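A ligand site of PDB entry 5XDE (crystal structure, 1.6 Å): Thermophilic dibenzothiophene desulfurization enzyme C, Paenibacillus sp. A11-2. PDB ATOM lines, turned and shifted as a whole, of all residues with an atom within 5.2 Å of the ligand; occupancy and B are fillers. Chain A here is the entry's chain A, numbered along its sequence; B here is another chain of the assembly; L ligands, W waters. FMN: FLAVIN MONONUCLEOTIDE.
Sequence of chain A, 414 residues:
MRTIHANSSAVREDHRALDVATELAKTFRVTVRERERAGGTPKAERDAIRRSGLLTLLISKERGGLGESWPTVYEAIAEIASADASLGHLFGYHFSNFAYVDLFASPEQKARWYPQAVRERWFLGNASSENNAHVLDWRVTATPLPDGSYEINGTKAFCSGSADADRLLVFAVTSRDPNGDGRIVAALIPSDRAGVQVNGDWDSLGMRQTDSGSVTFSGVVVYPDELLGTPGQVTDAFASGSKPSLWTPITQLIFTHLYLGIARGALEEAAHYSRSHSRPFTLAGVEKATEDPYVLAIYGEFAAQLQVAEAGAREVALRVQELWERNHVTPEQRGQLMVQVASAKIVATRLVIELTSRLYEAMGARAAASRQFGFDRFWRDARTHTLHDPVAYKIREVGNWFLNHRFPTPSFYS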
ATOM      1  N   HIS A  89      24.959   8.210 -20.570  1.00  0.00           N
ATOM      2  CA  HIS A  89      24.262   9.489 -20.501  1.00  0.00           C
ATOM      3  C   HIS A  89      24.940  10.529 -21.375  1.00  0.00           C
ATOM      4  O   HIS A  89      24.277  11.220 -22.164  1.00  0.00           O
ATOM      5  CB  HIS A  89      24.205   9.933 -19.041  1.00  0.00           C
ATOM      6  CG  HIS A  89      23.716  11.323 -18.825  1.00  0.00           C
ATOM      7  ND1 HIS A  89      22.444  11.606 -18.375  1.00  0.00           N
ATOM      8  CD2 HIS A  89      24.347  12.521 -18.943  1.00  0.00           C
ATOM      9  CE1 HIS A  89      22.315  12.906 -18.222  1.00  0.00           C
ATOM     10  NE2 HIS A  89      23.440  13.484 -18.587  1.00  0.00           N
ATOM     11  N   TYR A  93      23.198  12.136 -24.562  1.00  0.00           N
ATOM     12  CA  TYR A  93      22.904  13.562 -24.608  1.00  0.00           C
ATOM     13  C   TYR A  93      23.585  14.236 -25.786  1.00  0.00           C
ATOM     14  O   TYR A  93      23.055  15.210 -26.323  1.00  0.00           O
ATOM     15  CB  TYR A  93      23.330  14.258 -23.309  1.00  0.00           C
ATOM     16  CG  TYR A  93      22.301  14.199 -22.230  1.00  0.00           C
ATOM     17  CD1 TYR A  93      21.785  15.357 -21.676  1.00  0.00           C
ATOM     18  CD2 TYR A  93      21.817  12.974 -21.773  1.00  0.00           C
ATOM     19  CE1 TYR A  93      20.823  15.308 -20.685  1.00  0.00           C
ATOM     20  CE2 TYR A  93      20.861  12.917 -20.792  1.00  0.00           C
ATOM     21  CZ  TYR A  93      20.366  14.087 -20.234  1.00  0.00           C
ATOM     22  OH  TYR A  93      19.416  14.020 -19.231  1.00  0.00           O
ATOM     23  N   ASN A 126      25.661  20.687 -23.326  1.00  0.00           N
ATOM     24  CA  ASN A 126      24.583  21.665 -23.355  1.00  0.00           C
ATOM     25  C   ASN A 126      24.491  22.380 -22.022  1.00  0.00           C
ATOM     26  O   ASN A 126      24.864  21.841 -20.978  1.00  0.00           O
ATOM     27  CB  ASN A 126      23.228  21.014 -23.698  1.00  0.00           C
ATOM     28  CG  ASN A 126      22.632  20.287 -22.525  1.00  0.00           C
ATOM     29  OD1 ASN A 126      21.774  20.823 -21.809  1.00  0.00           O
ATOM     30  ND2 ASN A 126      23.103  19.060 -22.292  1.00  0.00           N
ATOM     31  N   SER A 128      21.278  24.392 -20.489  1.00  0.00           N
ATOM     32  CA  SER A 128      19.887  24.698 -20.829  1.00  0.00           C
ATOM     33  C   SER A 128      19.014  24.944 -19.610  1.00  0.00           C
ATOM     34  O   SER A 128      18.367  25.991 -19.496  1.00  0.00           O
ATOM     35  CB  SER A 128      19.308  23.555 -21.673  1.00  0.00           C
ATOM     36  OG  SER A 128      20.260  23.070 -22.603  1.00  0.00           O
ATOM     37  N   SER A 129      18.972  23.980 -18.686  1.00  0.00           N
ATOM     38  CA  SER A 129      18.127  24.086 -17.508  1.00  0.00           C
ATOM     39  C   SER A 129      18.781  24.989 -16.468  1.00  0.00           C
ATOM     40  O   SER A 129      19.984  25.274 -16.514  1.00  0.00           O
ATOM     41  CB  SER A 129      17.842  22.702 -16.914  1.00  0.00           C
ATOM     42  OG  SER A 129      17.060  21.920 -17.808  1.00  0.00           O
ATOM     43  N   VAL A 135      11.208  24.682 -13.022  1.00  0.00           N
ATOM     44  CA  VAL A 135      11.925  24.417 -14.269  1.00  0.00           C
ATOM     45  C   VAL A 135      11.660  25.483 -15.319  1.00  0.00           C
ATOM     46  O   VAL A 135      12.441  25.623 -16.261  1.00  0.00           O
ATOM     47  CB  VAL A 135      11.570  23.008 -14.806  1.00  0.00           C
ATOM     48  CG1 VAL A 135      12.359  21.930 -14.061  1.00  0.00           C
ATOM     49  CG2 VAL A 135      10.070  22.762 -14.700  1.00  0.00           C
ATOM     50  N   ALA A 157      22.202  25.266 -14.867  1.00  0.00           N
ATOM     51  CA  ALA A 157      22.386  24.093 -14.009  1.00  0.00           C
ATOM     52  C   ALA A 157      22.190  22.821 -14.820  1.00  0.00           C
ATOM     53  O   ALA A 157      21.648  22.841 -15.931  1.00  0.00           O
ATOM     54  CB  ALA A 157      21.421  24.111 -12.823  1.00  0.00           C
ATOM     55  N   PHE A 158      22.642  21.697 -14.250  1.00  0.00           N
ATOM     56  CA  PHE A 158      22.523  20.381 -14.860  1.00  0.00           C
ATOM     57  C   PHE A 158      23.039  20.374 -16.304  1.00  0.00           C
ATOM     58  O   PHE A 158      22.397  19.868 -17.225  1.00  0.00           O
ATOM     59  CB  PHE A 158      21.070  19.874 -14.807  1.00  0.00           C
ATOM     60  CG  PHE A 158      20.628  19.460 -13.434  1.00  0.00           C
ATOM     61  CD1 PHE A 158      21.025  18.236 -12.897  1.00  0.00           C
ATOM     62  CD2 PHE A 158      19.814  20.277 -12.675  1.00  0.00           C
ATOM     63  CE1 PHE A 158      20.610  17.846 -11.626  1.00  0.00           C
ATOM     64  CE2 PHE A 158      19.391  19.894 -11.404  1.00  0.00           C
ATOM     65  CZ  PHE A 158      19.792  18.675 -10.879  1.00  0.00           C
ATOM     66  N   CYS A 159      24.233  20.948 -16.485  1.00  0.00           N
ATOM     67  CA  CYS A 159      24.815  21.083 -17.823  1.00  0.00           C
ATOM     68  C   CYS A 159      25.593  19.808 -18.158  1.00  0.00           C
ATOM     69  O   CYS A 159      26.820  19.766 -18.147  1.00  0.00           O
ATOM     70  CB  CYS A 159      25.698  22.324 -17.894  1.00  0.00           C
ATOM     71  SG  CYS A 159      24.817  23.833 -17.449  1.00  0.00           S
ATOM     72  N   SER A 160      24.850  18.751 -18.459  1.00  0.00           N
ATOM     73  CA  SER A 160      25.467  17.463 -18.739  1.00  0.00           C
ATOM     74  C   SER A 160      26.510  17.606 -19.846  1.00  0.00           C
ATOM     75  O   SER A 160      26.274  18.253 -20.875  1.00  0.00           O
ATOM     76  CB  SER A 160      24.409  16.432 -19.140  1.00  0.00           C
ATOM     77  OG  SER A 160      23.701  15.985 -18.009  1.00  0.00           O
ATOM     78  N   TRP A 202      29.774  18.968  -9.690  1.00  0.00           N
ATOM     79  CA  TRP A 202      28.885  17.810  -9.769  1.00  0.00           C
ATOM     80  C   TRP A 202      29.378  16.747  -8.804  1.00  0.00           C
ATOM     81  O   TRP A 202      30.454  16.167  -8.995  1.00  0.00           O
ATOM     82  CB  TRP A 202      28.839  17.298 -11.206  1.00  0.00           C
ATOM     83  CG  TRP A 202      27.912  16.118 -11.480  1.00  0.00           C
ATOM     84  CD1 TRP A 202      28.285  14.885 -11.921  1.00  0.00           C
ATOM     85  CD2 TRP A 202      26.477  16.099 -11.367  1.00  0.00           C
ATOM     86  NE1 TRP A 202      27.176  14.081 -12.075  1.00  0.00           N
ATOM     87  CE2 TRP A 202      26.057  14.793 -11.746  1.00  0.00           C
ATOM     88  CE3 TRP A 202      25.509  17.031 -10.973  1.00  0.00           C
ATOM     89  CZ2 TRP A 202      24.703  14.414 -11.746  1.00  0.00           C
ATOM     90  CZ3 TRP A 202      24.168  16.653 -10.976  1.00  0.00           C
ATOM     91  CH2 TRP A 202      23.775  15.350 -11.361  1.00  0.00           C
ATOM     92  N   MET A 207      25.218   8.738 -11.432  1.00  0.00           N
ATOM     93  CA  MET A 207      25.575   9.549 -12.595  1.00  0.00           C
ATOM     94  C   MET A 207      26.767  10.448 -12.278  1.00  0.00           C
ATOM     95  O   MET A 207      26.842  11.618 -12.667  1.00  0.00           O
ATOM     96  CB  MET A 207      24.367  10.371 -13.076  1.00  0.00           C
ATOM     97  CG  MET A 207      23.139   9.507 -13.414  1.00  0.00           C
ATOM     98  SD  MET A 207      23.533   8.298 -14.670  1.00  0.00           S
ATOM     99  CE  MET A 207      21.941   7.712 -15.208  1.00  0.00           C
ATOM    100  N   THR A 210      28.926  12.480 -15.123  1.00  0.00           N
ATOM    101  CA  THR A 210      28.255  13.177 -16.223  1.00  0.00           C
ATOM    102  C   THR A 210      28.571  14.667 -16.273  1.00  0.00           C
ATOM    103  O   THR A 210      28.199  15.333 -17.248  1.00  0.00           O
ATOM    104  CB  THR A 210      26.722  13.004 -16.134  1.00  0.00           C
ATOM    105  OG1 THR A 210      26.227  13.552 -14.900  1.00  0.00           O
ATOM    106  CG2 THR A 210      26.331  11.542 -16.251  1.00  0.00           C
ATOM    107  N   SER A 212      27.320  17.168 -14.773  1.00  0.00           N
ATOM    108  CA  SER A 212      26.067  17.912 -14.890  1.00  0.00           C
ATOM    109  C   SER A 212      25.970  19.044 -13.883  1.00  0.00           C
ATOM    110  O   SER A 212      24.914  19.271 -13.299  1.00  0.00           O
ATOM    111  CB  SER A 212      24.882  16.964 -14.754  1.00  0.00           C
ATOM    112  OG  SER A 212      24.963  15.923 -15.724  1.00  0.00           O
ATOM    113  N   THR A 384      19.161   8.291  -9.513  1.00  0.00           N
ATOM    114  CA  THR A 384      19.481   9.698  -9.725  1.00  0.00           C
ATOM    115  C   THR A 384      18.841  10.204 -11.012  1.00  0.00           C
ATOM    116  O   THR A 384      18.146  11.229 -10.999  1.00  0.00           O
ATOM    117  CB  THR A 384      21.009   9.879  -9.762  1.00  0.00           C
ATOM    118  OG1 THR A 384      21.554   9.577  -8.474  1.00  0.00           O
ATOM    119  CG2 THR A 384      21.384  11.317 -10.145  1.00  0.00           C
ATOM    120  N   HIS A 385      19.027   9.482 -12.113  1.00  0.00           N
ATOM    121  CA  HIS A 385      18.625   9.998 -13.407  1.00  0.00           C
ATOM    122  C   HIS A 385      17.107  10.050 -13.550  1.00  0.00           C
ATOM    123  O   HIS A 385      16.563  10.994 -14.130  1.00  0.00           O
ATOM    124  CB  HIS A 385      19.233   9.167 -14.527  1.00  0.00           C
ATOM    125  CG  HIS A 385      19.227   9.865 -15.847  1.00  0.00           C
ATOM    126  ND1 HIS A 385      18.083  10.055 -16.585  1.00  0.00           N
ATOM    127  CD2 HIS A 385      20.230  10.436 -16.551  1.00  0.00           C
ATOM    128  CE1 HIS A 385      18.381  10.722 -17.689  1.00  0.00           C
ATOM    129  NE2 HIS A 385      19.683  10.955 -17.703  1.00  0.00           N
ATOM    130  N   LEU A 387      14.807  10.834 -11.827  1.00  0.00           N
ATOM    131  CA  LEU A 387      14.204  12.045 -11.317  1.00  0.00           C
ATOM    132  C   LEU A 387      14.382  13.216 -12.286  1.00  0.00           C
ATOM    133  O   LEU A 387      13.992  14.337 -11.945  1.00  0.00           O
ATOM    134  CB  LEU A 387      14.814  12.372  -9.953  1.00  0.00           C
ATOM    135  CG  LEU A 387      14.820  11.205  -8.938  1.00  0.00           C
ATOM    136  CD1 LEU A 387      15.667  11.503  -7.738  1.00  0.00           C
ATOM    137  CD2 LEU A 387      13.384  10.876  -8.508  1.00  0.00           C
ATOM    138  N   HIS A 388      14.937  12.952 -13.471  1.00  0.00           N
ATOM    139  CA  HIS A 388      15.186  13.990 -14.480  1.00  0.00           C
ATOM    140  C   HIS A 388      13.942  14.833 -14.710  1.00  0.00           C
ATOM    141  O   HIS A 388      13.995  16.065 -14.693  1.00  0.00           O
ATOM    142  CB  HIS A 388      15.662  13.341 -15.785  1.00  0.00           C
ATOM    143  CG  HIS A 388      16.196  14.303 -16.793  1.00  0.00           C
ATOM    144  ND1 HIS A 388      15.380  15.045 -17.625  1.00  0.00           N
ATOM    145  CD2 HIS A 388      17.472  14.649 -17.113  1.00  0.00           C
ATOM    146  CE1 HIS A 388      16.135  15.807 -18.409  1.00  0.00           C
ATOM    147  NE2 HIS A 388      17.399  15.585 -18.113  1.00  0.00           N
ATOM    148  N   ASP A 389      12.814  14.174 -14.981  1.00  0.00           N
ATOM    149  CA  ASP A 389      11.529  14.821 -14.959  1.00  0.00           C
ATOM    150  C   ASP A 389      10.587  13.827 -14.282  1.00  0.00           C
ATOM    151  O   ASP A 389      10.739  12.606 -14.455  1.00  0.00           O
ATOM    152  CB  ASP A 389      10.973  15.243 -16.340  1.00  0.00           C
ATOM    153  CG  ASP A 389      11.034  14.133 -17.365  1.00  0.00           C
ATOM    154  OD1 ASP A 389      12.102  13.939 -17.979  1.00  0.00           O
ATOM    155  OD2 ASP A 389       9.994  13.471 -17.601  1.00  0.00           O
ATOM    156  N   TYR A 413       9.589  19.352 -22.541  1.00  0.00           N
ATOM    157  CA  TYR A 413       9.377  18.209 -21.685  1.00  0.00           C
ATOM    158  C   TYR A 413       8.314  17.242 -22.180  1.00  0.00           C
ATOM    159  O   TYR A 413       8.267  16.103 -21.709  1.00  0.00           O
ATOM    160  CB  TYR A 413       9.027  18.671 -20.255  1.00  0.00           C
ATOM    161  CG  TYR A 413      10.076  19.583 -19.644  1.00  0.00           C
ATOM    162  CD1 TYR A 413      11.036  19.071 -18.769  1.00  0.00           C
ATOM    163  CD2 TYR A 413      10.119  20.934 -19.957  1.00  0.00           C
ATOM    164  CE1 TYR A 413      12.009  19.905 -18.211  1.00  0.00           C
ATOM    165  CE2 TYR A 413      11.083  21.773 -19.409  1.00  0.00           C
ATOM    166  CZ  TYR A 413      12.021  21.250 -18.538  1.00  0.00           C
ATOM    167  OH  TYR A 413      12.983  22.087 -18.000  1.00  0.00           O
ATOM    168  N   ARG B 279      10.871  21.648  -5.005  1.00  0.00           N
ATOM    169  CA  ARG B 279      10.314  22.673  -5.878  1.00  0.00           C
ATOM    170  C   ARG B 279       9.051  22.174  -6.567  1.00  0.00           C
ATOM    171  O   ARG B 279       9.013  21.018  -7.026  1.00  0.00           O
ATOM    172  CB  ARG B 279      11.331  23.103  -6.930  1.00  0.00           C
ATOM    173  CG  ARG B 279      12.463  23.961  -6.366  1.00  0.00           C
ATOM    174  CD  ARG B 279      13.809  23.703  -7.041  1.00  0.00           C
ATOM    175  NE  ARG B 279      13.915  24.285  -8.372  1.00  0.00           N
ATOM    176  CZ  ARG B 279      14.213  23.593  -9.480  1.00  0.00           C
ATOM    177  NH1 ARG B 279      14.425  22.289  -9.410  1.00  0.00           N
ATOM    178  NH2 ARG B 279      14.291  24.212 -10.646  1.00  0.00           N
ATOM    179  N   MET B 363      10.652  13.718  -3.361  1.00  0.00           N
ATOM    180  CA  MET B 363      11.571  14.801  -3.005  1.00  0.00           C
ATOM    181  C   MET B 363      12.107  15.551  -4.212  1.00  0.00           C
ATOM    182  O   MET B 363      12.291  16.768  -4.134  1.00  0.00           O
ATOM    183  CB  MET B 363      12.749  14.262  -2.177  1.00  0.00           C
ATOM    184  CG  MET B 363      12.375  13.836  -0.763  1.00  0.00           C
ATOM    185  SD  MET B 363      13.803  13.222   0.145  1.00  0.00           S
ATOM    186  CE  MET B 363      14.113  11.689  -0.714  1.00  0.00           C
ATOM    187  N   GLY B 364      12.385  14.865  -5.306  1.00  0.00           N
ATOM    188  CA  GLY B 364      12.852  15.495  -6.519  1.00  0.00           C
ATOM    189  C   GLY B 364      14.346  15.271  -6.753  1.00  0.00           C
ATOM    190  O   GLY B 364      15.074  14.774  -5.898  1.00  0.00           O
ATOM    191  N   ALA B 365      14.776  15.691  -7.939  1.00  0.00           N
ATOM    192  CA  ALA B 365      16.096  15.326  -8.445  1.00  0.00           C
ATOM    193  C   ALA B 365      17.225  15.872  -7.573  1.00  0.00           C
ATOM    194  O   ALA B 365      18.260  15.222  -7.442  1.00  0.00           O
ATOM    195  CB  ALA B 365      16.276  15.814  -9.886  1.00  0.00           C
ATOM    196  N   ARG B 366      17.049  17.055  -6.984  1.00  0.00           N
ATOM    197  CA  ARG B 366      18.155  17.610  -6.214  1.00  0.00           C
ATOM    198  C   ARG B 366      18.403  16.848  -4.917  1.00  0.00           C
ATOM    199  O   ARG B 366      19.467  17.017  -4.304  1.00  0.00           O
ATOM    200  CB  ARG B 366      17.896  19.093  -5.935  1.00  0.00           C
ATOM    201  CG  ARG B 366      18.094  19.965  -7.162  1.00  0.00           C
ATOM    202  CD  ARG B 366      16.911  20.887  -7.408  1.00  0.00           C
ATOM    203  NE  ARG B 366      16.712  21.817  -6.302  1.00  0.00           N
ATOM    204  CZ  ARG B 366      15.638  21.815  -5.505  1.00  0.00           C
ATOM    205  NH1 ARG B 366      14.663  20.942  -5.714  1.00  0.00           N
ATOM    206  NH2 ARG B 366      15.540  22.703  -4.525  1.00  0.00           N
HETATM  207  N1  FMN L   1      18.761  19.499 -17.763  1.00  0.00           N
HETATM  208  C2  FMN L   1      19.209  20.023 -18.951  1.00  0.00           C
HETATM  209  O2  FMN L   1      18.678  21.039 -19.403  1.00  0.00           O
HETATM  210  N3  FMN L   1      20.255  19.416 -19.639  1.00  0.00           N
HETATM  211  C4  FMN L   1      20.851  18.267 -19.123  1.00  0.00           C
HETATM  212  O4  FMN L   1      21.786  17.743 -19.743  1.00  0.00           O
HETATM  213  C4A FMN L   1      20.393  17.746 -17.913  1.00  0.00           C
HETATM  214  N5  FMN L   1      20.983  16.605 -17.387  1.00  0.00           N
HETATM  215  C5A FMN L   1      20.521  16.081 -16.196  1.00  0.00           C
HETATM  216  C6  FMN L   1      21.133  14.935 -15.673  1.00  0.00           C
HETATM  217  C7  FMN L   1      20.699  14.380 -14.471  1.00  0.00           C
HETATM  218  C7M FMN L   1      21.385  13.135 -13.955  1.00  0.00           C
HETATM  219  C8  FMN L   1      19.643  14.990 -13.793  1.00  0.00           C
HETATM  220  C8M FMN L   1      19.133  14.462 -12.489  1.00  0.00           C
HETATM  221  C9  FMN L   1      19.047  16.139 -14.309  1.00  0.00           C
HETATM  222  C9A FMN L   1      19.481  16.694 -15.511  1.00  0.00           C
HETATM  223  N10 FMN L   1      18.868  17.838 -16.043  1.00  0.00           N
HETATM  224  C10 FMN L   1      19.339  18.359 -17.225  1.00  0.00           C
HETATM  225  C1' FMN L   1      17.766  18.564 -15.284  1.00  0.00           C
HETATM  226  C2' FMN L   1      16.351  18.010 -15.282  1.00  0.00           C
HETATM  227  O2' FMN L   1      15.810  18.108 -16.584  1.00  0.00           O
HETATM  228  C3' FMN L   1      15.490  18.834 -14.298  1.00  0.00           C
HETATM  229  O3' FMN L   1      15.611  20.204 -14.610  1.00  0.00           O
HETATM  230  C4' FMN L   1      15.874  18.641 -12.824  1.00  0.00           C
HETATM  231  O4' FMN L   1      16.081  17.271 -12.575  1.00  0.00           O
HETATM  232  C5' FMN L   1      14.825  19.211 -11.860  1.00  0.00           C
HETATM  233  O5' FMN L   1      15.157  18.911 -10.511  1.00  0.00           O
HETATM  234  P   FMN L   1      14.037  18.861  -9.344  1.00  0.00           P
HETATM  235  O1P FMN L   1      13.236  17.575  -9.488  1.00  0.00           O
HETATM  236  O2P FMN L   1      14.680  18.906  -7.965  1.00  0.00           O
HETATM  237  O3P FMN L   1      13.126  20.057  -9.467  1.00  0.00           O
HETATM  238  O   HOH W   1      10.831  20.165 -10.331  1.00  0.00           O
HETATM  239  O   HOH W   2      12.281  19.493  -6.745  1.00  0.00           O
HETATM  240  O   HOH W   3      21.489  22.138 -18.543  1.00  0.00           O
HETATM  241  O   HOH W   4      14.811  21.648 -16.353  1.00  0.00           O
HETATM  242  O   HOH W   5      14.341  18.242  -5.270  1.00  0.00           O
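An oxygen (O2P) of the ligand lies within salt-bridge range of the guanidinium group (NH1) of Arg 366 of chain B (3.0 Å).
N5 of the ligand lies within hydrogen-bond range of OG of Ser 160 (2.9 Å).
The side-chain hydroxyl (OG) of Ser 129 sits at hydrogen-bond distance from an oxygen (O2) of the ligand (2.4 Å).
The backbone NH (N) of Ser 160 sits close to an oxygen (O4) of the ligand (3.5 Å).
The backbone carbonyl oxygen of Phe 158 sits close to a nitrogen (N3) of the ligand.
The backbone NH (N) of Ser 129 lies within hydrogen-bond range of an oxygen (O2) of the ligand, at 3.0 Å.
An oxygen (O4') of the ligand lies close to the backbone carbonyl oxygen of His 388 (3.2 Å).
The guanidinium group (NH1) of Arg 279 of chain B is in salt-bridge range of an oxygen (O3P) of the ligand (2.6 Å).
The backbone NH (N) of Arg 366 of chain B sits close to an oxygen (O2P) of the ligand, 3.2 Å away.
ND1 of His 388 lies close to O2' of the ligand, 3.3 Å away.
An oxygen (O1P) of the ligand is in hydrogen-bond range of the backbone NH of Ala 365 of chain B (2.9 Å).
A nitrogen (N3) of the ligand lies within hydrogen-bond range of the side-chain amide oxygen (OD1) of Asn 126.
A ring nitrogen (ND1) of His 89 sits at hydrogen-bond distance from a ring nitrogen (NE2) of His 385 (2.9 Å).
The side-chain hydroxyl of Ser 212 is in hydrogen-bond range of the side-chain hydroxyl of Thr 210.
The side-chain hydroxyl of Ser 160 lies within hydrogen-bond range of the side-chain hydroxyl of Ser 212, 2.6 Å away.
The side-chain hydroxyl (OG) of Ser 160 sits at hydrogen-bond distance from a ring nitrogen (NE2) of His 89.
A ring nitrogen (NE2) of His 385 lies within hydrogen-bond range of the side-chain hydroxyl of Tyr 93, 3.4 Å away.
The side-chain carboxylate (OD1) of Asp 389 is in hydrogen-bond range of a ring nitrogen (ND1) of His 388, 3.5 Å away.
N of Ala 157 is in hydrogen-bond range of O of Ser 129.
The backbone NH (N) of Phe 158 sits close to the backbone carbonyl oxygen (O) of Ser 212.
CE1 of His 89 touches C6 of the ligand (3.5 Å).
Tyr 93 touches the ligand.
Ser 128 touches the ligand (CB to O2, 3.4 Å).
CG1 of Val 135 touches O3' of the ligand (3.7 Å).
Ser 212 touches the ligand (OG to C6, 3.96 Å).
O of Thr 384 touches C8M of the ligand, at 3.7 Å.
CD2 of His 385 touches C7M of the ligand, at 3.9 Å.
Leu 387 touches the ligand.
CA of Gly 364 of chain B touches O1P of the ligand, 3.6 Å away.
Hydrophobic or aromatic side chains within 4 Å of the ligand: His 89, Tyr 93, Val 135, Phe 158, His 385, His 388 and Ala 365 of chain B.
Of the 25 residues printed, 17 come within 4 Å of the ligand.
The nearest printed residue that does not touch the ligand is Met 207 (4.1 Å).
Water W4 lies within hydrogen-bond range of O3' of the ligand (2.4 Å), OH of Tyr 413 (2.5 Å) and OG of Ser 129 (2.7 Å).
Water W2 lies within hydrogen-bond range of an oxygen (O2P) of the ligand (2.8 Å), the guanidinium group of Arg 366 of chain B (3.0 Å) and the backbone NH of Arg 279 of chain B (3.1 Å).
Water W5 lies within hydrogen-bond range of the guanidinium group of Arg 366 of chain B (2.8 Å), the backbone carbonyl oxygen of Met 363 of chain B (2.8 Å) and an oxygen (O2P) of the ligand (2.8 Å).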
